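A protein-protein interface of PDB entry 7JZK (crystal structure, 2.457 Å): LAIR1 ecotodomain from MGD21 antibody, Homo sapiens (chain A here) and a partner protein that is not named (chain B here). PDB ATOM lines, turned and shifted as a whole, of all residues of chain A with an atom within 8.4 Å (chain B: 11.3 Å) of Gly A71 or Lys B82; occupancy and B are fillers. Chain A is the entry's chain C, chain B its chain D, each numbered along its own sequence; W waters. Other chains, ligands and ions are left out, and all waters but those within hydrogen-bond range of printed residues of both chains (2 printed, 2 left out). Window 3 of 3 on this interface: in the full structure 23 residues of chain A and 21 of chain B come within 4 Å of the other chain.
The side-chain amide oxygen (OE1) of Gln B86 lies within hydrogen-bond range of the guanidinium group (NH2) of Arg A41 (3.1 Å). The side-chain amide nitrogen of Asn A72 lies within hydrogen-bond range of the backbone carbonyl oxygen of Phe B79, 2.8 Å away. N of Gly B81 lies close to ND2 of Asn A72.
N of Arg A39 sits at hydrogen-bond distance from O of Leu A44 (3.0 Å). The backbone carbonyl oxygen of Gly A71 is in hydrogen-bond range of the guanidinium group of Arg A39 (3.1 Å). O of Ala A73 is in hydrogen-bond range of NH2 of Arg A39, at 3.0 Å. The side-chain carboxylate of Glu A40 is in salt-bridge range of the guanidinium group of Arg A41 (2.9 Å). N of Asn A69 lies within hydrogen-bond range of OD1 of Asn A72. The side-chain sulfur of Cys B76 is disulfide-bonded to the side-chain sulfur of Cys B89, at 2.0 Å.
Among the printed residues, pairs that only touch across the chains: Arg A39 with Ala B78, Arg A39 with Gly B81, Leu A44 with Cys B76, Leu A44 with Gln B86, Leu A44 with Cys B89, Ile A65 with Phe B79, Gly A71 with Gly B81, Gly A71 with Lys B82, Asn A72 with Ser B80 and Phe A76 with Ala B78.
Of chain B, only Gly B81 (3.2 Å) and Lys B82 (3.8 Å) come within 4 Å of Gly A71. Lys B82 touches one residue of chain A. No residue of chain B comes within 4 Å of Asn A69. Ala A70 touches none of the printed residues of chain B. Asn A72 touches three residues of chain B. No residue of chain B comes within 4 Å of Ala A73. Gly B81 touches just these residues of chain A: Arg A39 (3.7 Å), Gly A71 (3.2 Å) and Asn A72 (3.4 Å). Of the printed residues of chain B, Arg A39 touches Ala B78 and Gly B81. Printed residues of chain A within 4 Å of Ala B78: Arg A39 (3.9 Å) and Phe A76 (3.5 Å). Printed residues of chain A within 4 Å of Ser B80: Asn A72. Of the printed residues of chain A, Cys B76 touches Leu A44 (3.6 Å). Of the printed residues of chain A, Gln B86 touches Arg A41 (3.1 Å) and Leu A44 (3.7 Å). The nearest printed residue of chain A that does not touch Ala B78 is Ile A65 (4.6 Å).
Hydrophobic or aromatic side chains of chain A that line the printed part of chain B: Leu A44, Ile A65 and Phe A76. Printed residues of chain B that touch a printed residue of chain A: Cys B76, Ala B78, Phe B79, Ser B80, Gly B81, Lys B82, Gln B86 and Cys B89. Among the printed residues, 13 pairs touch across the chains.
Water W1 lies within hydrogen-bond range of N of Lys B82, OD1 of Asn A69 and O of Ser B80. Water W2 lies within hydrogen-bond range of the side-chain amide nitrogen (NE2) of Gln B86 and the guanidinium group (NH1) of Arg A41.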
ATOM      1  N   LEU A  18      -8.025  -8.327  -7.578  1.00  0.00           N
ATOM      2  CA  LEU A  18      -9.168  -7.942  -6.767  1.00  0.00           C
ATOM      3  C   LEU A  18     -10.230  -9.022  -6.840  1.00  0.00           C
ATOM      4  O   LEU A  18     -10.579  -9.493  -7.926  1.00  0.00           O
ATOM      5  CB  LEU A  18      -9.730  -6.603  -7.267  1.00  0.00           C
ATOM      6  CG  LEU A  18     -10.795  -5.871  -6.425  1.00  0.00           C
ATOM      7  CD1 LEU A  18     -10.223  -5.411  -5.086  1.00  0.00           C
ATOM      8  CD2 LEU A  18     -11.407  -4.679  -7.176  1.00  0.00           C
ATOM      9  N   ARG A  39      -0.683  -7.261  11.209  1.00  0.00           N
ATOM     10  CA  ARG A  39      -0.642  -6.332  10.069  1.00  0.00           C
ATOM     11  C   ARG A  39       0.519  -5.370  10.283  1.00  0.00           C
ATOM     12  O   ARG A  39       1.370  -5.649  11.106  1.00  0.00           O
ATOM     13  CB  ARG A  39      -1.978  -5.605   9.943  1.00  0.00           C
ATOM     14  CG  ARG A  39      -3.159  -6.509   9.636  1.00  0.00           C
ATOM     15  CD  ARG A  39      -3.919  -5.968   8.447  1.00  0.00           C
ATOM     16  NE  ARG A  39      -3.042  -5.816   7.298  1.00  0.00           N
ATOM     17  CZ  ARG A  39      -3.423  -5.375   6.109  1.00  0.00           C
ATOM     18  NH1 ARG A  39      -4.681  -5.039   5.893  1.00  0.00           N
ATOM     19  NH2 ARG A  39      -2.540  -5.270   5.139  1.00  0.00           N
ATOM     20  N   GLU A  40       0.507  -4.252   9.590  1.00  0.00           N
ATOM     21  CA  GLU A  40       1.574  -3.234   9.730  1.00  0.00           C
ATOM     22  C   GLU A  40       1.611  -2.754  11.180  1.00  0.00           C
ATOM     23  O   GLU A  40       2.652  -2.283  11.613  1.00  0.00           O
ATOM     24  CB  GLU A  40       1.305  -2.097   8.754  1.00  0.00           C
ATOM     25  CG  GLU A  40       0.254  -2.426   7.713  1.00  0.00           C
ATOM     26  CD  GLU A  40      -1.175  -2.227   8.183  1.00  0.00           C
ATOM     27  OE1 GLU A  40      -1.370  -1.516   9.177  1.00  0.00           O
ATOM     28  OE2 GLU A  40      -2.079  -2.803   7.567  1.00  0.00           O
ATOM     29  N   ARG A  41       0.489  -2.857  11.880  1.00  0.00           N
ATOM     30  CA  ARG A  41       0.448  -2.467  13.295  1.00  0.00           C
ATOM     31  C   ARG A  41       0.262  -3.664  14.217  1.00  0.00           C
ATOM     32  O   ARG A  41      -0.517  -4.548  13.871  1.00  0.00           O
ATOM     33  CB  ARG A  41      -0.435  -1.240  13.502  1.00  0.00           C
ATOM     34  CG  ARG A  41       0.258   0.063  13.139  1.00  0.00           C
ATOM     35  CD  ARG A  41      -0.677   1.091  12.544  1.00  0.00           C
ATOM     36  NE  ARG A  41      -1.505   0.553  11.478  1.00  0.00           N
ATOM     37  CZ  ARG A  41      -2.358   1.274  10.762  1.00  0.00           C
ATOM     38  NH1 ARG A  41      -3.079   0.703   9.812  1.00  0.00           N
ATOM     39  NH2 ARG A  41      -2.490   2.564  11.003  1.00  0.00           N
ATOM     40  N   LEU A  44      -3.287  -4.817  15.331  1.00  0.00           N
ATOM     41  CA  LEU A  44      -4.202  -5.418  14.342  1.00  0.00           C
ATOM     42  C   LEU A  44      -3.698  -6.832  14.076  1.00  0.00           C
ATOM     43  O   LEU A  44      -2.654  -6.981  13.443  1.00  0.00           O
ATOM     44  CB  LEU A  44      -4.214  -4.531  13.102  1.00  0.00           C
ATOM     45  CG  LEU A  44      -4.488  -3.055  13.355  1.00  0.00           C
ATOM     46  CD1 LEU A  44      -4.235  -2.241  12.099  1.00  0.00           C
ATOM     47  CD2 LEU A  44      -5.909  -2.851  13.841  1.00  0.00           C
ATOM     48  N   ILE A  65      -7.740 -15.471   3.213  1.00  0.00           N
ATOM     49  CA  ILE A  65      -8.744 -14.499   2.808  1.00  0.00           C
ATOM     50  C   ILE A  65      -9.368 -14.992   1.507  1.00  0.00           C
ATOM     51  O   ILE A  65      -8.671 -15.118   0.492  1.00  0.00           O
ATOM     52  CB  ILE A  65      -8.136 -13.094   2.628  1.00  0.00           C
ATOM     53  CG1 ILE A  65      -7.528 -12.572   3.931  1.00  0.00           C
ATOM     54  CG2 ILE A  65      -9.197 -12.123   2.107  1.00  0.00           C
ATOM     55  CD1 ILE A  65      -6.800 -11.257   3.742  1.00  0.00           C
ATOM     56  N   VAL A  68     -10.150 -10.853  -1.519  1.00  0.00           N
ATOM     57  CA  VAL A  68      -9.446  -9.668  -1.053  1.00  0.00           C
ATOM     58  C   VAL A  68     -10.083  -8.420  -1.642  1.00  0.00           C
ATOM     59  O   VAL A  68     -10.653  -8.439  -2.740  1.00  0.00           O
ATOM     60  CB  VAL A  68      -7.947  -9.731  -1.399  1.00  0.00           C
ATOM     61  CG1 VAL A  68      -7.346 -11.033  -0.902  1.00  0.00           C
ATOM     62  CG2 VAL A  68      -7.743  -9.546  -2.893  1.00  0.00           C
ATOM     63  N   ASN A  69     -10.004  -7.330  -0.896  1.00  0.00           N
ATOM     64  CA  ASN A  69     -10.323  -6.006  -1.415  1.00  0.00           C
ATOM     65  C   ASN A  69      -9.109  -5.119  -1.179  1.00  0.00           C
ATOM     66  O   ASN A  69      -8.089  -5.570  -0.633  1.00  0.00           O
ATOM     67  CB  ASN A  69     -11.591  -5.417  -0.785  1.00  0.00           C
ATOM     68  CG  ASN A  69     -11.560  -5.415   0.726  1.00  0.00           C
ATOM     69  OD1 ASN A  69     -10.679  -4.812   1.351  1.00  0.00           O
ATOM     70  ND2 ASN A  69     -12.539  -6.078   1.330  1.00  0.00           N
ATOM     71  N   ALA A  70      -9.228  -3.850  -1.604  1.00  0.00           N
ATOM     72  CA  ALA A  70      -8.086  -2.941  -1.523  1.00  0.00           C
ATOM     73  C   ALA A  70      -7.597  -2.761  -0.089  1.00  0.00           C
ATOM     74  O   ALA A  70      -6.400  -2.535   0.127  1.00  0.00           O
ATOM     75  CB  ALA A  70      -8.448  -1.576  -2.122  1.00  0.00           C
ATOM     76  N   GLY A  71      -8.487  -2.898   0.899  1.00  0.00           N
ATOM     77  CA  GLY A  71      -8.083  -2.746   2.284  1.00  0.00           C
ATOM     78  C   GLY A  71      -7.204  -3.865   2.796  1.00  0.00           C
ATOM     79  O   GLY A  71      -6.530  -3.693   3.817  1.00  0.00           O
ATOM     80  N   ASN A  72      -7.225  -5.021   2.147  1.00  0.00           N
ATOM     81  CA  ASN A  72      -6.357  -6.106   2.576  1.00  0.00           C
ATOM     82  C   ASN A  72      -4.906  -5.878   2.183  1.00  0.00           C
ATOM     83  O   ASN A  72      -4.020  -6.513   2.768  1.00  0.00           O
ATOM     84  CB  ASN A  72      -6.821  -7.430   1.978  1.00  0.00           C
ATOM     85  CG  ASN A  72      -8.150  -7.876   2.510  1.00  0.00           C
ATOM     86  OD1 ASN A  72      -9.083  -8.114   1.746  1.00  0.00           O
ATOM     87  ND2 ASN A  72      -8.250  -8.003   3.826  1.00  0.00           N
ATOM     88  N   ALA A  73      -4.651  -4.998   1.208  1.00  0.00           N
ATOM     89  CA  ALA A  73      -3.297  -4.735   0.728  1.00  0.00           C
ATOM     90  C   ALA A  73      -2.412  -4.197   1.853  1.00  0.00           C
ATOM     91  O   ALA A  73      -2.872  -3.468   2.741  1.00  0.00           O
ATOM     92  CB  ALA A  73      -3.332  -3.741  -0.435  1.00  0.00           C
ATOM     93  N   GLY A  74      -1.118  -4.566   1.826  1.00  0.00           N
ATOM     94  CA  GLY A  74      -0.246  -4.008   2.837  1.00  0.00           C
ATOM     95  C   GLY A  74       0.639  -5.073   3.456  1.00  0.00           C
ATOM     96  O   GLY A  74       0.838  -6.148   2.898  1.00  0.00           O
ATOM     97  N   LEU A  75       1.157  -4.795   4.642  1.00  0.00           N
ATOM     98  CA  LEU A  75       2.103  -5.672   5.315  1.00  0.00           C
ATOM     99  C   LEU A  75       1.467  -6.662   6.298  1.00  0.00           C
ATOM    100  O   LEU A  75       0.504  -6.337   6.986  1.00  0.00           O
ATOM    101  CB  LEU A  75       3.143  -4.808   6.028  1.00  0.00           C
ATOM    102  CG  LEU A  75       4.308  -4.203   5.218  1.00  0.00           C
ATOM    103  CD1 LEU A  75       3.931  -3.606   3.891  1.00  0.00           C
ATOM    104  CD2 LEU A  75       5.081  -3.220   6.045  1.00  0.00           C
ATOM    105  N   PHE A  76       2.034  -7.878   6.345  1.00  0.00           N
ATOM    106  CA  PHE A  76       1.650  -8.979   7.226  1.00  0.00           C
ATOM    107  C   PHE A  76       2.917  -9.649   7.749  1.00  0.00           C
ATOM    108  O   PHE A  76       3.936  -9.680   7.061  1.00  0.00           O
ATOM    109  CB  PHE A  76       0.791 -10.059   6.520  1.00  0.00           C
ATOM    110  CG  PHE A  76      -0.536  -9.555   5.994  1.00  0.00           C
ATOM    111  CD1 PHE A  76      -0.614  -8.924   4.751  1.00  0.00           C
ATOM    112  CD2 PHE A  76      -1.713  -9.723   6.733  1.00  0.00           C
ATOM    113  CE1 PHE A  76      -1.830  -8.470   4.261  1.00  0.00           C
ATOM    114  CE2 PHE A  76      -2.934  -9.274   6.241  1.00  0.00           C
ATOM    115  CZ  PHE A  76      -2.992  -8.642   5.008  1.00  0.00           C
ATOM    116  N   LEU A  95       1.472  -7.551   0.603  1.00  0.00           N
ATOM    117  CA  LEU A  95       0.427  -8.075  -0.258  1.00  0.00           C
ATOM    118  C   LEU A  95      -0.006  -6.964  -1.198  1.00  0.00           C
ATOM    119  O   LEU A  95      -0.377  -5.873  -0.748  1.00  0.00           O
ATOM    120  CB  LEU A  95      -0.765  -8.577   0.557  1.00  0.00           C
ATOM    121  CG  LEU A  95      -2.041  -8.791  -0.261  1.00  0.00           C
ATOM    122  CD1 LEU A  95      -1.862  -9.982  -1.181  1.00  0.00           C
ATOM    123  CD2 LEU A  95      -3.247  -8.981   0.632  1.00  0.00           C
ATOM    124  N   VAL A  97      -2.680  -6.039  -4.178  1.00  0.00           N
ATOM    125  CA  VAL A  97      -3.953  -6.381  -4.811  1.00  0.00           C
ATOM    126  C   VAL A  97      -4.103  -5.523  -6.062  1.00  0.00           C
ATOM    127  O   VAL A  97      -3.866  -4.307  -6.026  1.00  0.00           O
ATOM    128  CB  VAL A  97      -5.143  -6.188  -3.854  1.00  0.00           C
ATOM    129  CG1 VAL A  97      -5.097  -4.822  -3.238  1.00  0.00           C
ATOM    130  CG2 VAL A  97      -6.474  -6.358  -4.589  1.00  0.00           C
ATOM    131  N   ALA B  74     -13.277  -8.938  16.967  1.00  0.00           N
ATOM    132  CA  ALA B  74     -13.916  -8.859  15.652  1.00  0.00           C
ATOM    133  C   ALA B  74     -13.491  -7.656  14.807  1.00  0.00           C
ATOM    134  O   ALA B  74     -13.549  -7.733  13.571  1.00  0.00           O
ATOM    135  CB  ALA B  74     -15.432  -8.853  15.811  1.00  0.00           C
ATOM    136  N   SER B  75     -13.085  -6.539  15.414  1.00  0.00           N
ATOM    137  CA  SER B  75     -12.854  -5.319  14.642  1.00  0.00           C
ATOM    138  C   SER B  75     -11.380  -4.937  14.508  1.00  0.00           C
ATOM    139  O   SER B  75     -11.078  -3.890  13.914  1.00  0.00           O
ATOM    140  CB  SER B  75     -13.655  -4.143  15.233  1.00  0.00           C
ATOM    141  OG  SER B  75     -13.586  -4.088  16.645  1.00  0.00           O
ATOM    142  N   CYS B  76     -10.461  -5.732  15.052  1.00  0.00           N
ATOM    143  CA  CYS B  76      -9.035  -5.442  15.007  1.00  0.00           C
ATOM    144  C   CYS B  76      -8.278  -6.657  14.509  1.00  0.00           C
ATOM    145  O   CYS B  76      -7.270  -7.068  15.084  1.00  0.00           O
ATOM    146  CB  CYS B  76      -8.506  -5.053  16.375  1.00  0.00           C
ATOM    147  SG  CYS B  76      -9.435  -3.749  17.128  1.00  0.00           S
ATOM    148  N   ASP B  77      -8.739  -7.244  13.414  1.00  0.00           N
ATOM    149  CA  ASP B  77      -8.191  -8.505  12.934  1.00  0.00           C
ATOM    150  C   ASP B  77      -7.349  -8.328  11.675  1.00  0.00           C
ATOM    151  O   ASP B  77      -7.329  -7.268  11.040  1.00  0.00           O
ATOM    152  CB  ASP B  77      -9.303  -9.519  12.648  1.00  0.00           C
ATOM    153  CG  ASP B  77     -10.236  -9.078  11.531  1.00  0.00           C
ATOM    154  OD1 ASP B  77     -10.809  -7.961  11.588  1.00  0.00           O
ATOM    155  OD2 ASP B  77     -10.334  -9.835  10.541  1.00  0.00           O
ATOM    156  N   ALA B  78      -6.657  -9.419  11.306  1.00  0.00           N
ATOM    157  CA  ALA B  78      -5.780  -9.407  10.147  1.00  0.00           C
ATOM    158  C   ALA B  78      -6.540  -9.636   8.844  1.00  0.00           C
ATOM    159  O   ALA B  78      -6.030  -9.283   7.778  1.00  0.00           O
ATOM    160  CB  ALA B  78      -4.667 -10.464  10.324  1.00  0.00           C
ATOM    161  N   PHE B  79      -7.737 -10.225   8.905  1.00  0.00           N
ATOM    162  CA  PHE B  79      -8.535 -10.551   7.719  1.00  0.00           C
ATOM    163  C   PHE B  79      -9.346  -9.381   7.166  1.00  0.00           C
ATOM    164  O   PHE B  79      -9.541  -9.296   5.951  1.00  0.00           O
ATOM    165  CB  PHE B  79      -9.529 -11.666   8.048  1.00  0.00           C
ATOM    166  CG  PHE B  79      -8.896 -12.959   8.411  1.00  0.00           C
ATOM    167  CD1 PHE B  79      -8.806 -13.352   9.736  1.00  0.00           C
ATOM    168  CD2 PHE B  79      -8.343 -13.770   7.429  1.00  0.00           C
ATOM    169  CE1 PHE B  79      -8.199 -14.564  10.079  1.00  0.00           C
ATOM    170  CE2 PHE B  79      -7.745 -14.982   7.758  1.00  0.00           C
ATOM    171  CZ  PHE B  79      -7.670 -15.374   9.086  1.00  0.00           C
ATOM    172  N   SER B  80      -9.847  -8.493   8.027  1.00  0.00           N
ATOM    173  CA  SER B  80     -10.925  -7.586   7.620  1.00  0.00           C
ATOM    174  C   SER B  80     -10.507  -6.496   6.641  1.00  0.00           C
ATOM    175  O   SER B  80     -11.378  -5.918   5.987  1.00  0.00           O
ATOM    176  CB  SER B  80     -11.553  -6.925   8.848  1.00  0.00           C
ATOM    177  OG  SER B  80     -12.478  -5.936   8.456  1.00  0.00           O
ATOM    178  N   GLY B  81      -9.238  -6.185   6.547  1.00  0.00           N
ATOM    179  CA  GLY B  81      -8.781  -5.128   5.648  1.00  0.00           C
ATOM    180  C   GLY B  81      -8.615  -3.788   6.394  1.00  0.00           C
ATOM    181  O   GLY B  81      -7.802  -3.695   7.297  1.00  0.00           O
ATOM    182  N   LYS B  82      -9.437  -2.820   6.040  1.00  0.00           N
ATOM    183  CA  LYS B  82      -9.267  -1.491   6.615  1.00  0.00           C
ATOM    184  C   LYS B  82     -10.023  -1.380   7.930  1.00  0.00           C
ATOM    185  O   LYS B  82     -11.209  -1.706   7.986  1.00  0.00           O
ATOM    186  CB  LYS B  82      -9.764  -0.422   5.649  1.00  0.00           C
ATOM    187  CG  LYS B  82      -9.567   0.955   6.230  1.00  0.00           C
ATOM    188  CD  LYS B  82     -10.189   2.051   5.381  1.00  0.00           C
ATOM    189  CE  LYS B  82     -10.254   3.351   6.163  1.00  0.00           C
ATOM    190  NZ  LYS B  82     -11.094   4.354   5.456  1.00  0.00           N
ATOM    191  N   ILE B  83      -9.343  -0.924   8.982  1.00  0.00           N
ATOM    192  CA  ILE B  83      -9.989  -0.757  10.275  1.00  0.00           C
ATOM    193  C   ILE B  83     -10.248   0.723  10.447  1.00  0.00           C
ATOM    194  O   ILE B  83      -9.315   1.524  10.480  1.00  0.00           O
ATOM    195  CB  ILE B  83      -9.155  -1.308  11.440  1.00  0.00           C
ATOM    196  CG1 ILE B  83      -9.151  -2.840  11.459  1.00  0.00           C
ATOM    197  CG2 ILE B  83      -9.670  -0.798  12.797  1.00  0.00           C
ATOM    198  CD1 ILE B  83      -8.134  -3.477  10.563  1.00  0.00           C
ATOM    199  N   VAL B  84     -11.527   1.090  10.498  1.00  0.00           N
ATOM    200  CA  VAL B  84     -11.903   2.501  10.574  1.00  0.00           C
ATOM    201  C   VAL B  84     -11.456   3.106  11.901  1.00  0.00           C
ATOM    202  O   VAL B  84     -10.873   4.190  11.932  1.00  0.00           O
ATOM    203  CB  VAL B  84     -13.416   2.690  10.342  1.00  0.00           C
ATOM    204  CG1 VAL B  84     -13.817   4.118  10.650  1.00  0.00           C
ATOM    205  CG2 VAL B  84     -13.810   2.293   8.915  1.00  0.00           C
ATOM    206  N   ASN B  85     -11.676   2.360  12.994  1.00  0.00           N
ATOM    207  CA  ASN B  85     -11.383   2.767  14.396  1.00  0.00           C
ATOM    208  C   ASN B  85     -10.058   2.206  14.923  1.00  0.00           C
ATOM    209  O   ASN B  85     -10.097   1.196  15.604  1.00  0.00           O
ATOM    210  CB  ASN B  85     -12.559   2.539  15.347  1.00  0.00           C
ATOM    211  CG  ASN B  85     -12.421   3.195  16.703  1.00  0.00           C
ATOM    212  OD1 ASN B  85     -11.352   3.642  17.093  1.00  0.00           O
ATOM    213  ND2 ASN B  85     -13.514   3.245  17.436  1.00  0.00           N
ATOM    214  N   GLN B  86      -8.939   2.798  14.561  1.00  0.00           N
ATOM    215  CA  GLN B  86      -7.614   2.391  15.071  1.00  0.00           C
ATOM    216  C   GLN B  86      -7.467   2.618  16.581  1.00  0.00           C
ATOM    217  O   GLN B  86      -6.797   1.816  17.206  1.00  0.00           O
ATOM    218  CB  GLN B  86      -6.548   3.081  14.228  1.00  0.00           C
ATOM    219  CG  GLN B  86      -6.649   2.740  12.752  1.00  0.00           C
ATOM    220  CD  GLN B  86      -5.692   1.640  12.373  1.00  0.00           C
ATOM    221  OE1 GLN B  86      -4.645   1.470  12.986  1.00  0.00           O
ATOM    222  NE2 GLN B  86      -6.041   0.891  11.341  1.00  0.00           N
ATOM    223  N   ALA B  87      -8.031   3.673  17.137  1.00  0.00           N
ATOM    224  CA  ALA B  87      -7.856   4.012  18.562  1.00  0.00           C
ATOM    225  C   ALA B  87      -8.354   2.897  19.474  1.00  0.00           C
ATOM    226  O   ALA B  87      -7.746   2.682  20.520  1.00  0.00           O
ATOM    227  CB  ALA B  87      -8.559   5.294  18.849  1.00  0.00           C
ATOM    228  N   PHE B  88      -9.453   2.265  19.108  1.00  0.00           N
ATOM    229  CA  PHE B  88      -9.971   1.120  19.859  1.00  0.00           C
ATOM    230  C   PHE B  88      -8.971  -0.030  19.866  1.00  0.00           C
ATOM    231  O   PHE B  88      -8.639  -0.566  20.919  1.00  0.00           O
ATOM    232  CB  PHE B  88     -11.305   0.670  19.243  1.00  0.00           C
ATOM    233  CG  PHE B  88     -11.940  -0.520  19.911  1.00  0.00           C
ATOM    234  CD1 PHE B  88     -11.969  -0.633  21.294  1.00  0.00           C
ATOM    235  CD2 PHE B  88     -12.553  -1.501  19.157  1.00  0.00           C
ATOM    236  CE1 PHE B  88     -12.598  -1.727  21.909  1.00  0.00           C
ATOM    237  CE2 PHE B  88     -13.171  -2.602  19.769  1.00  0.00           C
ATOM    238  CZ  PHE B  88     -13.185  -2.712  21.144  1.00  0.00           C
ATOM    239  N   CYS B  89      -8.418  -0.365  18.706  1.00  0.00           N
ATOM    240  CA  CYS B  89      -7.437  -1.439  18.637  1.00  0.00           C
ATOM    241  C   CYS B  89      -6.149  -1.050  19.354  1.00  0.00           C
ATOM    242  O   CYS B  89      -5.540  -1.886  20.023  1.00  0.00           O
ATOM    243  CB  CYS B  89      -7.181  -1.766  17.161  1.00  0.00           C
ATOM    244  SG  CYS B  89      -8.740  -2.047  16.272  1.00  0.00           S
HETATM  245  O   HOH W   1     -11.027  -3.009   4.199  1.00  0.00           O
HETATM  246  O   HOH W   2      -5.796  -0.542   8.523  1.00  0.00           O
